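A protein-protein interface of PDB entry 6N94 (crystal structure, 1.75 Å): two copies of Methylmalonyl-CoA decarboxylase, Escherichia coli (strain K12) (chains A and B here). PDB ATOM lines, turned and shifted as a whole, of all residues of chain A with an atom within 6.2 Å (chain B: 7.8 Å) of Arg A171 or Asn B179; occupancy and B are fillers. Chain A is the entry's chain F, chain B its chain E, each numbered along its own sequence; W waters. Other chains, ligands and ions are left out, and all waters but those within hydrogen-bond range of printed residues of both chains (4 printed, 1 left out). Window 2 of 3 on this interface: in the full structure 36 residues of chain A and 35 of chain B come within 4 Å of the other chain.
Positions printed for both chains: 172, 173, 176 and 177. Of the 15 pairs that touch across the chains among the printed residues, none has its exchanged pair printed and touching as well.
Of the 18 printed residues of chain A, 6 touch a printed residue of chain B. Hydrophobic or aromatic side chains of chain A that line the printed part of chain B: Phe A154, His A155 and Ile A156. Hydrophobic or aromatic side chains of chain B that line the printed part of chain A: Leu B120, Ile B121, His B180 and Met B194. Among the printed residues, 15 pairs touch across the chains.
O of Ser B118 lies within hydrogen-bond range of NE2 of His A155 (3.2 Å). The side-chain carboxylate (OD1) of Asp B119 is in salt-bridge range of the side-chain amino group (NZ) of Lys A158, at 2.8 Å. OD1 of Asp B151 sits at hydrogen-bond distance from N of Phe A154, 3.1 Å away. OD1 of Asp B151 is in hydrogen-bond range of N of His A155 (2.8 Å). The backbone carbonyl oxygen (O) of Ile B177 sits at hydrogen-bond distance from a ring nitrogen (ND1) of His A155 (2.7 Å). The side-chain amide nitrogen (ND2) of Asn B179 is in hydrogen-bond range of the backbone carbonyl oxygen (O) of His A155, 2.9 Å away. The side-chain carboxylate (OE1) of Glu A159 lies within hydrogen-bond range of the side-chain amide nitrogen (ND2) of Asn B179 (2.9 Å). The backbone carbonyl oxygen (O) of Asn B179 lies within hydrogen-bond range of the guanidinium group (NH2) of Arg A171, 3.1 Å away. The side-chain carboxylate of Glu A159 sits at hydrogen-bond distance from a ring nitrogen (NE2) of His B180 (2.8 Å).
Among the printed residues, merely in contact across the chains: His A155 with Asp B119 (3.4 Å), His A155 with Ile B121 (3.5 Å), Ile A156 with Asn B179 (3.8 Å), Glu A159 with Leu B120 (3.7 Å), Glu A159 with Met B194 (3.7 Å) and Arg A171 with His B180 (3.7 Å).
Water W1 bridges the side-chain carboxylate of Asp B119 and the side-chain amino group of Lys A158. Water W3 lies within hydrogen-bond range of the side-chain carboxylate (OD1) of Asp B151, the backbone carbonyl oxygen (O) of Gly B176, the backbone NH (N) of Ile A156 and the backbone NH (N) of His A155. Water W4 lies within hydrogen-bond range of the side-chain carboxylate of Asp B151 (2.7 Å) and a ring nitrogen (NE2) of His A155 (3.2 Å). Water W2 lies within hydrogen-bond range of O of Ser B118 (2.8 Å) and NZ of Lys A158 (2.8 Å).
N of Ser B101 sits at hydrogen-bond distance from O of Leu B120. The backbone carbonyl oxygen (O) of Leu B120 is in hydrogen-bond range of the side-chain hydroxyl (OG) of Ser B118 (3.5 Å). The side-chain amide oxygen (OD1) of Asn B179 sits at hydrogen-bond distance from the backbone NH (N) of Ile B121 (2.9 Å). The backbone carbonyl oxygen (O) of His B180 is in hydrogen-bond range of the backbone NH (N) of Ala B123 (3.0 Å). NH2 of Arg A171 is in salt-bridge range of OE1 of Glu A159, 2.8 Å away. The side-chain hydroxyl of Thr A168 lies within hydrogen-bond range of the backbone NH of Arg A171 (3.0 Å).
Of the printed residues of chain B, Phe A154 touches Asp B151. Of chain B, only Asn B179 (3.1 Å) and His B180 (3.7 Å) come within 4 Å of Arg A171. Printed residues of chain A within 4 Å of Ile B177: His A155. Printed residues of chain A within 4 Å of Asn B179: His A155 (2.9 Å), Ile A156 (3.8 Å), Glu A159 (2.9 Å) and Arg A171 (3.1 Å). Of the printed residues of chain A, Met B194 touches Glu A159 (3.7 Å). The nearest printed residue of chain A that does not touch Asn B179 is Lys A158 (5.7 Å).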
ATOM      1  N   PHE A 154      16.921 -11.377 -23.293  1.00  0.00           N
ATOM      2  CA  PHE A 154      17.959 -10.628 -22.561  1.00  0.00           C
ATOM      3  C   PHE A 154      17.587  -9.147 -22.455  1.00  0.00           C
ATOM      4  O   PHE A 154      17.725  -8.554 -21.371  1.00  0.00           O
ATOM      5  CB  PHE A 154      19.300 -10.761 -23.282  1.00  0.00           C
ATOM      6  CG  PHE A 154      20.298 -11.656 -22.608  1.00  0.00           C
ATOM      7  CD1 PHE A 154      19.886 -12.770 -21.919  1.00  0.00           C
ATOM      8  CD2 PHE A 154      21.649 -11.375 -22.691  1.00  0.00           C
ATOM      9  CE1 PHE A 154      20.798 -13.572 -21.269  1.00  0.00           C
ATOM     10  CE2 PHE A 154      22.570 -12.206 -22.074  1.00  0.00           C
ATOM     11  CZ  PHE A 154      22.131 -13.285 -21.362  1.00  0.00           C
ATOM     12  N   HIS A 155      17.157  -8.505 -23.538  1.00  0.00           N
ATOM     13  CA  HIS A 155      16.824  -7.055 -23.446  1.00  0.00           C
ATOM     14  C   HIS A 155      15.719  -6.833 -22.401  1.00  0.00           C
ATOM     15  O   HIS A 155      15.792  -5.847 -21.600  1.00  0.00           O
ATOM     16  CB  HIS A 155      16.435  -6.489 -24.815  1.00  0.00           C
ATOM     17  CG  HIS A 155      17.489  -6.600 -25.865  1.00  0.00           C
ATOM     18  ND1 HIS A 155      17.173  -6.619 -27.203  1.00  0.00           N
ATOM     19  CD2 HIS A 155      18.843  -6.671 -25.784  1.00  0.00           C
ATOM     20  CE1 HIS A 155      18.285  -6.733 -27.916  1.00  0.00           C
ATOM     21  NE2 HIS A 155      19.343  -6.759 -27.048  1.00  0.00           N
ATOM     22  N   ILE A 156      14.700  -7.658 -22.389  1.00  0.00           N
ATOM     23  CA  ILE A 156      13.575  -7.524 -21.415  1.00  0.00           C
ATOM     24  C   ILE A 156      14.103  -7.742 -19.996  1.00  0.00           C
ATOM     25  O   ILE A 156      13.793  -6.922 -19.077  1.00  0.00           O
ATOM     26  CB  ILE A 156      12.419  -8.477 -21.743  1.00  0.00           C
ATOM     27  CG1 ILE A 156      11.836  -8.187 -23.120  1.00  0.00           C
ATOM     28  CG2 ILE A 156      11.344  -8.393 -20.670  1.00  0.00           C
ATOM     29  CD1 ILE A 156      11.296  -6.785 -23.273  1.00  0.00           C
ATOM     30  N   VAL A 157      14.906  -8.780 -19.793  1.00  0.00           N
ATOM     31  CA  VAL A 157      15.414  -9.052 -18.427  1.00  0.00           C
ATOM     32  C   VAL A 157      16.264  -7.863 -17.951  1.00  0.00           C
ATOM     33  O   VAL A 157      16.147  -7.446 -16.786  1.00  0.00           O
ATOM     34  CB  VAL A 157      16.163 -10.399 -18.426  1.00  0.00           C
ATOM     35  CG1 VAL A 157      16.999 -10.618 -17.182  1.00  0.00           C
ATOM     36  CG2 VAL A 157      15.138 -11.502 -18.628  1.00  0.00           C
ATOM     37  N   LYS A 158      17.127  -7.310 -18.813  1.00  0.00           N
ATOM     38  CA  LYS A 158      17.989  -6.189 -18.435  1.00  0.00           C
ATOM     39  C   LYS A 158      17.158  -4.938 -18.109  1.00  0.00           C
ATOM     40  O   LYS A 158      17.471  -4.262 -17.121  1.00  0.00           O
ATOM     41  CB  LYS A 158      19.042  -5.943 -19.522  1.00  0.00           C
ATOM     42  CG  LYS A 158      20.173  -6.968 -19.536  1.00  0.00           C
ATOM     43  CD  LYS A 158      20.887  -6.884 -20.892  1.00  0.00           C
ATOM     44  CE  LYS A 158      22.012  -7.819 -21.099  1.00  0.00           C
ATOM     45  NZ  LYS A 158      22.947  -7.360 -22.149  1.00  0.00           N
ATOM     46  N   GLU A 159      16.075  -4.671 -18.850  1.00  0.00           N
ATOM     47  CA  GLU A 159      15.162  -3.563 -18.483  1.00  0.00           C
ATOM     48  C   GLU A 159      14.579  -3.818 -17.081  1.00  0.00           C
ATOM     49  O   GLU A 159      14.620  -2.883 -16.242  1.00  0.00           O
ATOM     50  CB  GLU A 159      14.014  -3.414 -19.486  1.00  0.00           C
ATOM     51  CG  GLU A 159      13.028  -2.323 -19.070  1.00  0.00           C
ATOM     52  CD  GLU A 159      11.822  -2.180 -19.998  1.00  0.00           C
ATOM     53  OE1 GLU A 159      11.808  -2.834 -21.073  1.00  0.00           O
ATOM     54  OE2 GLU A 159      10.866  -1.499 -19.590  1.00  0.00           O
ATOM     55  N   LEU A 160      14.076  -5.014 -16.802  1.00  0.00           N
ATOM     56  CA  LEU A 160      13.471  -5.328 -15.482  1.00  0.00           C
ATOM     57  C   LEU A 160      14.486  -5.101 -14.352  1.00  0.00           C
ATOM     58  O   LEU A 160      14.163  -4.440 -13.319  1.00  0.00           O
ATOM     59  CB  LEU A 160      13.043  -6.799 -15.460  1.00  0.00           C
ATOM     60  CG  LEU A 160      11.772  -7.149 -16.208  1.00  0.00           C
ATOM     61  CD1 LEU A 160      11.518  -8.640 -16.062  1.00  0.00           C
ATOM     62  CD2 LEU A 160      10.601  -6.357 -15.625  1.00  0.00           C
ATOM     63  N   ILE A 167       6.403  -4.304 -13.595  1.00  0.00           N
ATOM     64  CA  ILE A 167       5.578  -4.558 -14.800  1.00  0.00           C
ATOM     65  C   ILE A 167       4.217  -5.141 -14.389  1.00  0.00           C
ATOM     66  O   ILE A 167       4.104  -5.847 -13.351  1.00  0.00           O
ATOM     67  CB  ILE A 167       6.307  -5.457 -15.795  1.00  0.00           C
ATOM     68  CG1 ILE A 167       6.584  -6.828 -15.208  1.00  0.00           C
ATOM     69  CG2 ILE A 167       7.589  -4.791 -16.290  1.00  0.00           C
ATOM     70  CD1 ILE A 167       7.002  -7.824 -16.260  1.00  0.00           C
ATOM     71  N   THR A 168       3.242  -4.928 -15.266  1.00  0.00           N
ATOM     72  CA  THR A 168       1.870  -5.472 -15.125  1.00  0.00           C
ATOM     73  C   THR A 168       1.861  -6.962 -15.449  1.00  0.00           C
ATOM     74  O   THR A 168       2.749  -7.409 -16.159  1.00  0.00           O
ATOM     75  CB  THR A 168       0.917  -4.730 -16.077  1.00  0.00           C
ATOM     76  OG1 THR A 168       1.292  -4.961 -17.421  1.00  0.00           O
ATOM     77  CG2 THR A 168       0.881  -3.238 -15.795  1.00  0.00           C
ATOM     78  N   ALA A 169       0.816  -7.659 -15.015  1.00  0.00           N
ATOM     79  CA  ALA A 169       0.501  -9.038 -15.424  1.00  0.00           C
ATOM     80  C   ALA A 169       0.371  -9.102 -16.937  1.00  0.00           C
ATOM     81  O   ALA A 169       0.860 -10.073 -17.528  1.00  0.00           O
ATOM     82  CB  ALA A 169      -0.758  -9.515 -14.710  1.00  0.00           C
ATOM     83  N   GLN A 170      -0.199  -8.080 -17.579  1.00  0.00           N
ATOM     84  CA  GLN A 170      -0.418  -8.118 -19.044  1.00  0.00           C
ATOM     85  C   GLN A 170       0.933  -8.061 -19.749  1.00  0.00           C
ATOM     86  O   GLN A 170       1.164  -8.894 -20.711  1.00  0.00           O
ATOM     87  CB  GLN A 170      -1.334  -6.983 -19.498  1.00  0.00           C
ATOM     88  CG  GLN A 170      -2.755  -7.146 -18.952  1.00  0.00           C
ATOM     89  CD  GLN A 170      -2.908  -6.794 -17.490  1.00  0.00           C
ATOM     90  OE1 GLN A 170      -2.131  -6.024 -16.952  1.00  0.00           O
ATOM     91  NE2 GLN A 170      -3.967  -7.311 -16.858  1.00  0.00           N
ATOM     92  N   ARG A 171       1.837  -7.219 -19.270  1.00  0.00           N
ATOM     93  CA  ARG A 171       3.179  -7.174 -19.927  1.00  0.00           C
ATOM     94  C   ARG A 171       3.955  -8.468 -19.606  1.00  0.00           C
ATOM     95  O   ARG A 171       4.672  -8.959 -20.506  1.00  0.00           O
ATOM     96  CB  ARG A 171       4.027  -5.993 -19.503  1.00  0.00           C
ATOM     97  CG  ARG A 171       5.270  -5.840 -20.378  1.00  0.00           C
ATOM     98  CD  ARG A 171       6.053  -4.583 -20.223  1.00  0.00           C
ATOM     99  NE  ARG A 171       7.191  -4.538 -21.154  1.00  0.00           N
ATOM    100  CZ  ARG A 171       8.310  -3.915 -20.908  1.00  0.00           C
ATOM    101  NH1 ARG A 171       8.457  -3.246 -19.778  1.00  0.00           N
ATOM    102  NH2 ARG A 171       9.283  -3.903 -21.816  1.00  0.00           N
ATOM    103  N   ALA A 172       3.891  -8.974 -18.371  1.00  0.00           N
ATOM    104  CA  ALA A 172       4.594 -10.234 -18.019  1.00  0.00           C
ATOM    105  C   ALA A 172       4.122 -11.409 -18.901  1.00  0.00           C
ATOM    106  O   ALA A 172       4.936 -12.254 -19.294  1.00  0.00           O
ATOM    107  CB  ALA A 172       4.392 -10.508 -16.557  1.00  0.00           C
ATOM    108  N   LEU A 173       2.825 -11.481 -19.224  1.00  0.00           N
ATOM    109  CA  LEU A 173       2.275 -12.460 -20.185  1.00  0.00           C
ATOM    110  C   LEU A 173       2.903 -12.261 -21.572  1.00  0.00           C
ATOM    111  O   LEU A 173       3.322 -13.257 -22.181  1.00  0.00           O
ATOM    112  CB  LEU A 173       0.747 -12.325 -20.225  1.00  0.00           C
ATOM    113  CG  LEU A 173       0.058 -13.381 -21.085  1.00  0.00           C
ATOM    114  CD1 LEU A 173       0.120 -14.751 -20.393  1.00  0.00           C
ATOM    115  CD2 LEU A 173      -1.389 -13.004 -21.355  1.00  0.00           C
ATOM    116  N   ALA A 174       2.888 -11.038 -22.070  1.00  0.00           N
ATOM    117  CA  ALA A 174       3.359 -10.663 -23.424  1.00  0.00           C
ATOM    118  C   ALA A 174       4.839 -11.079 -23.600  1.00  0.00           C
ATOM    119  O   ALA A 174       5.200 -11.623 -24.679  1.00  0.00           O
ATOM    120  CB  ALA A 174       3.156  -9.180 -23.623  1.00  0.00           C
ATOM    121  N   VAL A 175       5.660 -10.897 -22.577  1.00  0.00           N
ATOM    122  CA  VAL A 175       7.144 -11.091 -22.749  1.00  0.00           C
ATOM    123  C   VAL A 175       7.515 -12.554 -22.448  1.00  0.00           C
ATOM    124  O   VAL A 175       8.685 -12.908 -22.621  1.00  0.00           O
ATOM    125  CB  VAL A 175       7.957 -10.087 -21.912  1.00  0.00           C
ATOM    126  CG1 VAL A 175       7.589  -8.639 -22.231  1.00  0.00           C
ATOM    127  CG2 VAL A 175       7.852 -10.313 -20.410  1.00  0.00           C
ATOM    128  N   GLY A 176       6.578 -13.404 -21.986  1.00  0.00           N
ATOM    129  CA  GLY A 176       6.829 -14.847 -21.779  1.00  0.00           C
ATOM    130  C   GLY A 176       7.065 -15.283 -20.335  1.00  0.00           C
ATOM    131  O   GLY A 176       7.321 -16.497 -20.099  1.00  0.00           O
ATOM    132  N   ILE A 177       6.897 -14.388 -19.364  1.00  0.00           N
ATOM    133  CA  ILE A 177       7.101 -14.707 -17.942  1.00  0.00           C
ATOM    134  C   ILE A 177       5.936 -15.529 -17.385  1.00  0.00           C
ATOM    135  O   ILE A 177       6.204 -16.501 -16.649  1.00  0.00           O
ATOM    136  CB  ILE A 177       7.356 -13.417 -17.143  1.00  0.00           C
ATOM    137  CG1 ILE A 177       8.746 -12.857 -17.470  1.00  0.00           C
ATOM    138  CG2 ILE A 177       7.207 -13.668 -15.665  1.00  0.00           C
ATOM    139  CD1 ILE A 177       8.809 -11.395 -17.182  1.00  0.00           C
ATOM    140  N   ILE B 100      21.836   1.827 -24.053  1.00  0.00           N
ATOM    141  CA  ILE B 100      20.492   1.807 -24.690  1.00  0.00           C
ATOM    142  C   ILE B 100      20.646   2.255 -26.140  1.00  0.00           C
ATOM    143  O   ILE B 100      21.203   3.351 -26.380  1.00  0.00           O
ATOM    144  CB  ILE B 100      19.453   2.675 -23.958  1.00  0.00           C
ATOM    145  CG1 ILE B 100      19.321   2.308 -22.484  1.00  0.00           C
ATOM    146  CG2 ILE B 100      18.094   2.653 -24.684  1.00  0.00           C
ATOM    147  CD1 ILE B 100      18.574   3.337 -21.692  1.00  0.00           C
ATOM    148  N   SER B 101      20.226   1.420 -27.091  1.00  0.00           N
ATOM    149  CA  SER B 101      20.130   1.809 -28.512  1.00  0.00           C
ATOM    150  C   SER B 101      18.782   2.485 -28.703  1.00  0.00           C
ATOM    151  O   SER B 101      17.747   1.850 -28.405  1.00  0.00           O
ATOM    152  CB  SER B 101      20.275   0.614 -29.428  1.00  0.00           C
ATOM    153  OG  SER B 101      21.588   0.131 -29.311  1.00  0.00           O
ATOM    154  N   SER B 118      23.621  -4.450 -27.543  1.00  0.00           N
ATOM    155  CA  SER B 118      23.375  -3.464 -26.475  1.00  0.00           C
ATOM    156  C   SER B 118      22.345  -4.023 -25.475  1.00  0.00           C
ATOM    157  O   SER B 118      21.781  -5.114 -25.715  1.00  0.00           O
ATOM    158  CB  SER B 118      22.987  -2.090 -27.042  1.00  0.00           C
ATOM    159  OG  SER B 118      21.671  -2.068 -27.620  1.00  0.00           O
ATOM    160  N   ASP B 119      22.118  -3.300 -24.376  1.00  0.00           N
ATOM    161  CA  ASP B 119      21.340  -3.796 -23.211  1.00  0.00           C
ATOM    162  C   ASP B 119      19.833  -3.633 -23.444  1.00  0.00           C
ATOM    163  O   ASP B 119      19.063  -4.534 -23.032  1.00  0.00           O
ATOM    164  CB  ASP B 119      21.883  -3.173 -21.924  1.00  0.00           C
ATOM    165  CG  ASP B 119      23.376  -3.437 -21.797  1.00  0.00           C
ATOM    166  OD1 ASP B 119      23.753  -4.651 -21.829  1.00  0.00           O
ATOM    167  OD2 ASP B 119      24.157  -2.464 -21.708  1.00  0.00           O
ATOM    168  N   LEU B 120      19.398  -2.493 -24.010  1.00  0.00           N
ATOM    169  CA  LEU B 120      17.959  -2.207 -24.220  1.00  0.00           C
ATOM    170  C   LEU B 120      17.846  -1.557 -25.589  1.00  0.00           C
ATOM    171  O   LEU B 120      18.824  -0.908 -26.025  1.00  0.00           O
ATOM    172  CB  LEU B 120      17.465  -1.229 -23.144  1.00  0.00           C
ATOM    173  CG  LEU B 120      17.041  -1.773 -21.789  1.00  0.00           C
ATOM    174  CD1 LEU B 120      18.262  -1.891 -20.876  1.00  0.00           C
ATOM    175  CD2 LEU B 120      16.014  -0.838 -21.153  1.00  0.00           C
ATOM    176  N   ILE B 121      16.730  -1.778 -26.281  1.00  0.00           N
ATOM    177  CA  ILE B 121      16.437  -1.121 -27.582  1.00  0.00           C
ATOM    178  C   ILE B 121      15.073  -0.440 -27.455  1.00  0.00           C
ATOM    179  O   ILE B 121      14.081  -1.075 -27.124  1.00  0.00           O
ATOM    180  CB  ILE B 121      16.477  -2.053 -28.796  1.00  0.00           C
ATOM    181  CG1 ILE B 121      17.724  -2.932 -28.842  1.00  0.00           C
ATOM    182  CG2 ILE B 121      16.352  -1.236 -30.062  1.00  0.00           C
ATOM    183  CD1 ILE B 121      17.684  -3.981 -29.952  1.00  0.00           C
ATOM    184  N   ILE B 122      15.057   0.864 -27.676  1.00  0.00           N
ATOM    185  CA  ILE B 122      13.814   1.667 -27.695  1.00  0.00           C
ATOM    186  C   ILE B 122      13.755   2.288 -29.088  1.00  0.00           C
ATOM    187  O   ILE B 122      14.782   2.853 -29.535  1.00  0.00           O
ATOM    188  CB  ILE B 122      13.862   2.726 -26.571  1.00  0.00           C
ATOM    189  CG1 ILE B 122      14.026   2.074 -25.205  1.00  0.00           C
ATOM    190  CG2 ILE B 122      12.613   3.581 -26.640  1.00  0.00           C
ATOM    191  CD1 ILE B 122      14.121   3.017 -24.089  1.00  0.00           C
ATOM    192  N   ALA B 123      12.660   2.089 -29.808  1.00  0.00           N
ATOM    193  CA  ALA B 123      12.596   2.444 -31.233  1.00  0.00           C
ATOM    194  C   ALA B 123      11.322   3.224 -31.588  1.00  0.00           C
ATOM    195  O   ALA B 123      10.216   3.001 -31.003  1.00  0.00           O
ATOM    196  CB  ALA B 123      12.686   1.181 -32.048  1.00  0.00           C
ATOM    197  N   ASP B 151      17.182 -13.028 -27.746  1.00  0.00           N
ATOM    198  CA  ASP B 151      15.943 -12.240 -27.588  1.00  0.00           C
ATOM    199  C   ASP B 151      14.771 -12.975 -28.255  1.00  0.00           C
ATOM    200  O   ASP B 151      13.896 -13.450 -27.537  1.00  0.00           O
ATOM    201  CB  ASP B 151      16.238 -10.816 -28.060  1.00  0.00           C
ATOM    202  CG  ASP B 151      17.263 -10.128 -27.175  1.00  0.00           C
ATOM    203  OD1 ASP B 151      16.878  -9.783 -25.998  1.00  0.00           O
ATOM    204  OD2 ASP B 151      18.471  -9.959 -27.665  1.00  0.00           O
ATOM    205  N   ALA B 172       9.047  -6.469 -34.317  1.00  0.00           N
ATOM    206  CA  ALA B 172      10.288  -6.585 -33.516  1.00  0.00           C
ATOM    207  C   ALA B 172       9.948  -6.516 -32.026  1.00  0.00           C
ATOM    208  O   ALA B 172      10.527  -7.291 -31.236  1.00  0.00           O
ATOM    209  CB  ALA B 172      11.325  -5.592 -33.971  1.00  0.00           C
ATOM    210  N   LEU B 173       8.934  -5.743 -31.641  1.00  0.00           N
ATOM    211  CA  LEU B 173       8.428  -5.727 -30.253  1.00  0.00           C
ATOM    212  C   LEU B 173       7.768  -7.073 -29.908  1.00  0.00           C
ATOM    213  O   LEU B 173       8.054  -7.621 -28.820  1.00  0.00           O
ATOM    214  CB  LEU B 173       7.457  -4.570 -30.055  1.00  0.00           C
ATOM    215  CG  LEU B 173       6.905  -4.401 -28.642  1.00  0.00           C
ATOM    216  CD1 LEU B 173       7.946  -3.889 -27.650  1.00  0.00           C
ATOM    217  CD2 LEU B 173       5.712  -3.441 -28.703  1.00  0.00           C
ATOM    218  N   GLY B 176      10.132 -10.030 -29.265  1.00  0.00           N
ATOM    219  CA  GLY B 176      11.037  -9.821 -28.119  1.00  0.00           C
ATOM    220  C   GLY B 176      12.373  -9.175 -28.449  1.00  0.00           C
ATOM    221  O   GLY B 176      13.201  -9.068 -27.489  1.00  0.00           O
ATOM    222  N   ILE B 177      12.588  -8.664 -29.670  1.00  0.00           N
ATOM    223  CA  ILE B 177      13.826  -7.920 -30.020  1.00  0.00           C
ATOM    224  C   ILE B 177      13.853  -6.551 -29.285  1.00  0.00           C
ATOM    225  O   ILE B 177      14.928  -6.144 -28.717  1.00  0.00           O
ATOM    226  CB  ILE B 177      13.909  -7.817 -31.546  1.00  0.00           C
ATOM    227  CG1 ILE B 177      14.245  -9.194 -32.142  1.00  0.00           C
ATOM    228  CG2 ILE B 177      14.859  -6.713 -31.991  1.00  0.00           C
ATOM    229  CD1 ILE B 177      13.986  -9.292 -33.591  1.00  0.00           C
ATOM    230  N   LEU B 178      12.739  -5.832 -29.262  1.00  0.00           N
ATOM    231  CA  LEU B 178      12.681  -4.449 -28.728  1.00  0.00           C
ATOM    232  C   LEU B 178      12.091  -4.444 -27.322  1.00  0.00           C
ATOM    233  O   LEU B 178      11.256  -5.284 -26.997  1.00  0.00           O
ATOM    234  CB  LEU B 178      11.833  -3.529 -29.630  1.00  0.00           C
ATOM    235  CG  LEU B 178      12.259  -3.376 -31.081  1.00  0.00           C
ATOM    236  CD1 LEU B 178      11.273  -2.509 -31.852  1.00  0.00           C
ATOM    237  CD2 LEU B 178      13.648  -2.794 -31.174  1.00  0.00           C
ATOM    238  N   ASN B 179      12.469  -3.447 -26.532  1.00  0.00           N
ATOM    239  CA  ASN B 179      11.853  -3.157 -25.212  1.00  0.00           C
ATOM    240  C   ASN B 179      10.571  -2.348 -25.363  1.00  0.00           C
ATOM    241  O   ASN B 179       9.563  -2.681 -24.704  1.00  0.00           O
ATOM    242  CB  ASN B 179      12.812  -2.427 -24.290  1.00  0.00           C
ATOM    243  CG  ASN B 179      13.972  -3.325 -23.908  1.00  0.00           C
ATOM    244  OD1 ASN B 179      14.931  -3.440 -24.693  1.00  0.00           O
ATOM    245  ND2 ASN B 179      13.902  -3.929 -22.723  1.00  0.00           N
ATOM    246  N   HIS B 180      10.648  -1.269 -26.097  1.00  0.00           N
ATOM    247  CA  HIS B 180       9.519  -0.337 -26.289  1.00  0.00           C
ATOM    248  C   HIS B 180       9.521   0.222 -27.706  1.00  0.00           C
ATOM    249  O   HIS B 180      10.629   0.431 -28.306  1.00  0.00           O
ATOM    250  CB  HIS B 180       9.631   0.820 -25.306  1.00  0.00           C
ATOM    251  CG  HIS B 180       9.490   0.400 -23.897  1.00  0.00           C
ATOM    252  ND1 HIS B 180       8.245   0.145 -23.320  1.00  0.00           N
ATOM    253  CD2 HIS B 180      10.425   0.163 -22.960  1.00  0.00           C
ATOM    254  CE1 HIS B 180       8.446  -0.219 -22.078  1.00  0.00           C
ATOM    255  NE2 HIS B 180       9.771  -0.245 -21.837  1.00  0.00           N
ATOM    256  N   VAL B 181       8.311   0.499 -28.195  1.00  0.00           N
ATOM    257  CA  VAL B 181       8.083   1.242 -29.451  1.00  0.00           C
ATOM    258  C   VAL B 181       7.323   2.518 -29.098  1.00  0.00           C
ATOM    259  O   VAL B 181       6.353   2.422 -28.389  1.00  0.00           O
ATOM    260  CB  VAL B 181       7.329   0.394 -30.478  1.00  0.00           C
ATOM    261  CG1 VAL B 181       6.986   1.230 -31.710  1.00  0.00           C
ATOM    262  CG2 VAL B 181       8.174  -0.841 -30.847  1.00  0.00           C
ATOM    263  N   PHE B 190      11.225   9.865 -23.885  1.00  0.00           N
ATOM    264  CA  PHE B 190      10.926   8.530 -23.284  1.00  0.00           C
ATOM    265  C   PHE B 190      12.236   7.838 -22.885  1.00  0.00           C
ATOM    266  O   PHE B 190      12.354   7.359 -21.758  1.00  0.00           O
ATOM    267  CB  PHE B 190      10.168   7.623 -24.259  1.00  0.00           C
ATOM    268  CG  PHE B 190       9.742   6.305 -23.675  1.00  0.00           C
ATOM    269  CD1 PHE B 190      10.574   5.198 -23.749  1.00  0.00           C
ATOM    270  CD2 PHE B 190       8.506   6.159 -23.061  1.00  0.00           C
ATOM    271  CE1 PHE B 190      10.197   3.993 -23.167  1.00  0.00           C
ATOM    272  CE2 PHE B 190       8.123   4.947 -22.503  1.00  0.00           C
ATOM    273  CZ  PHE B 190       8.969   3.856 -22.564  1.00  0.00           C
ATOM    274  N   MET B 194      13.935   7.102 -18.963  1.00  0.00           N
ATOM    275  CA  MET B 194      14.367   5.764 -18.510  1.00  0.00           C
ATOM    276  C   MET B 194      15.854   5.781 -18.125  1.00  0.00           C
ATOM    277  O   MET B 194      16.193   5.187 -17.060  1.00  0.00           O
ATOM    278  CB  MET B 194      14.098   4.686 -19.565  1.00  0.00           C
ATOM    279  CG  MET B 194      14.284   3.263 -18.961  1.00  0.00           C
ATOM    280  SD  MET B 194      13.773   2.000 -20.103  1.00  0.00           S
ATOM    281  CE  MET B 194      11.999   2.025 -19.910  1.00  0.00           C
HETATM  282  O   HOH W   1      25.313  -5.737 -23.546  1.00  0.00           O
HETATM  283  O   HOH W   2      21.964  -7.718 -24.761  1.00  0.00           O
HETATM  284  O   HOH W   3      14.397  -9.405 -25.017  1.00  0.00           O
HETATM  285  O   HOH W   4      20.734  -9.578 -26.226  1.00  0.00           O
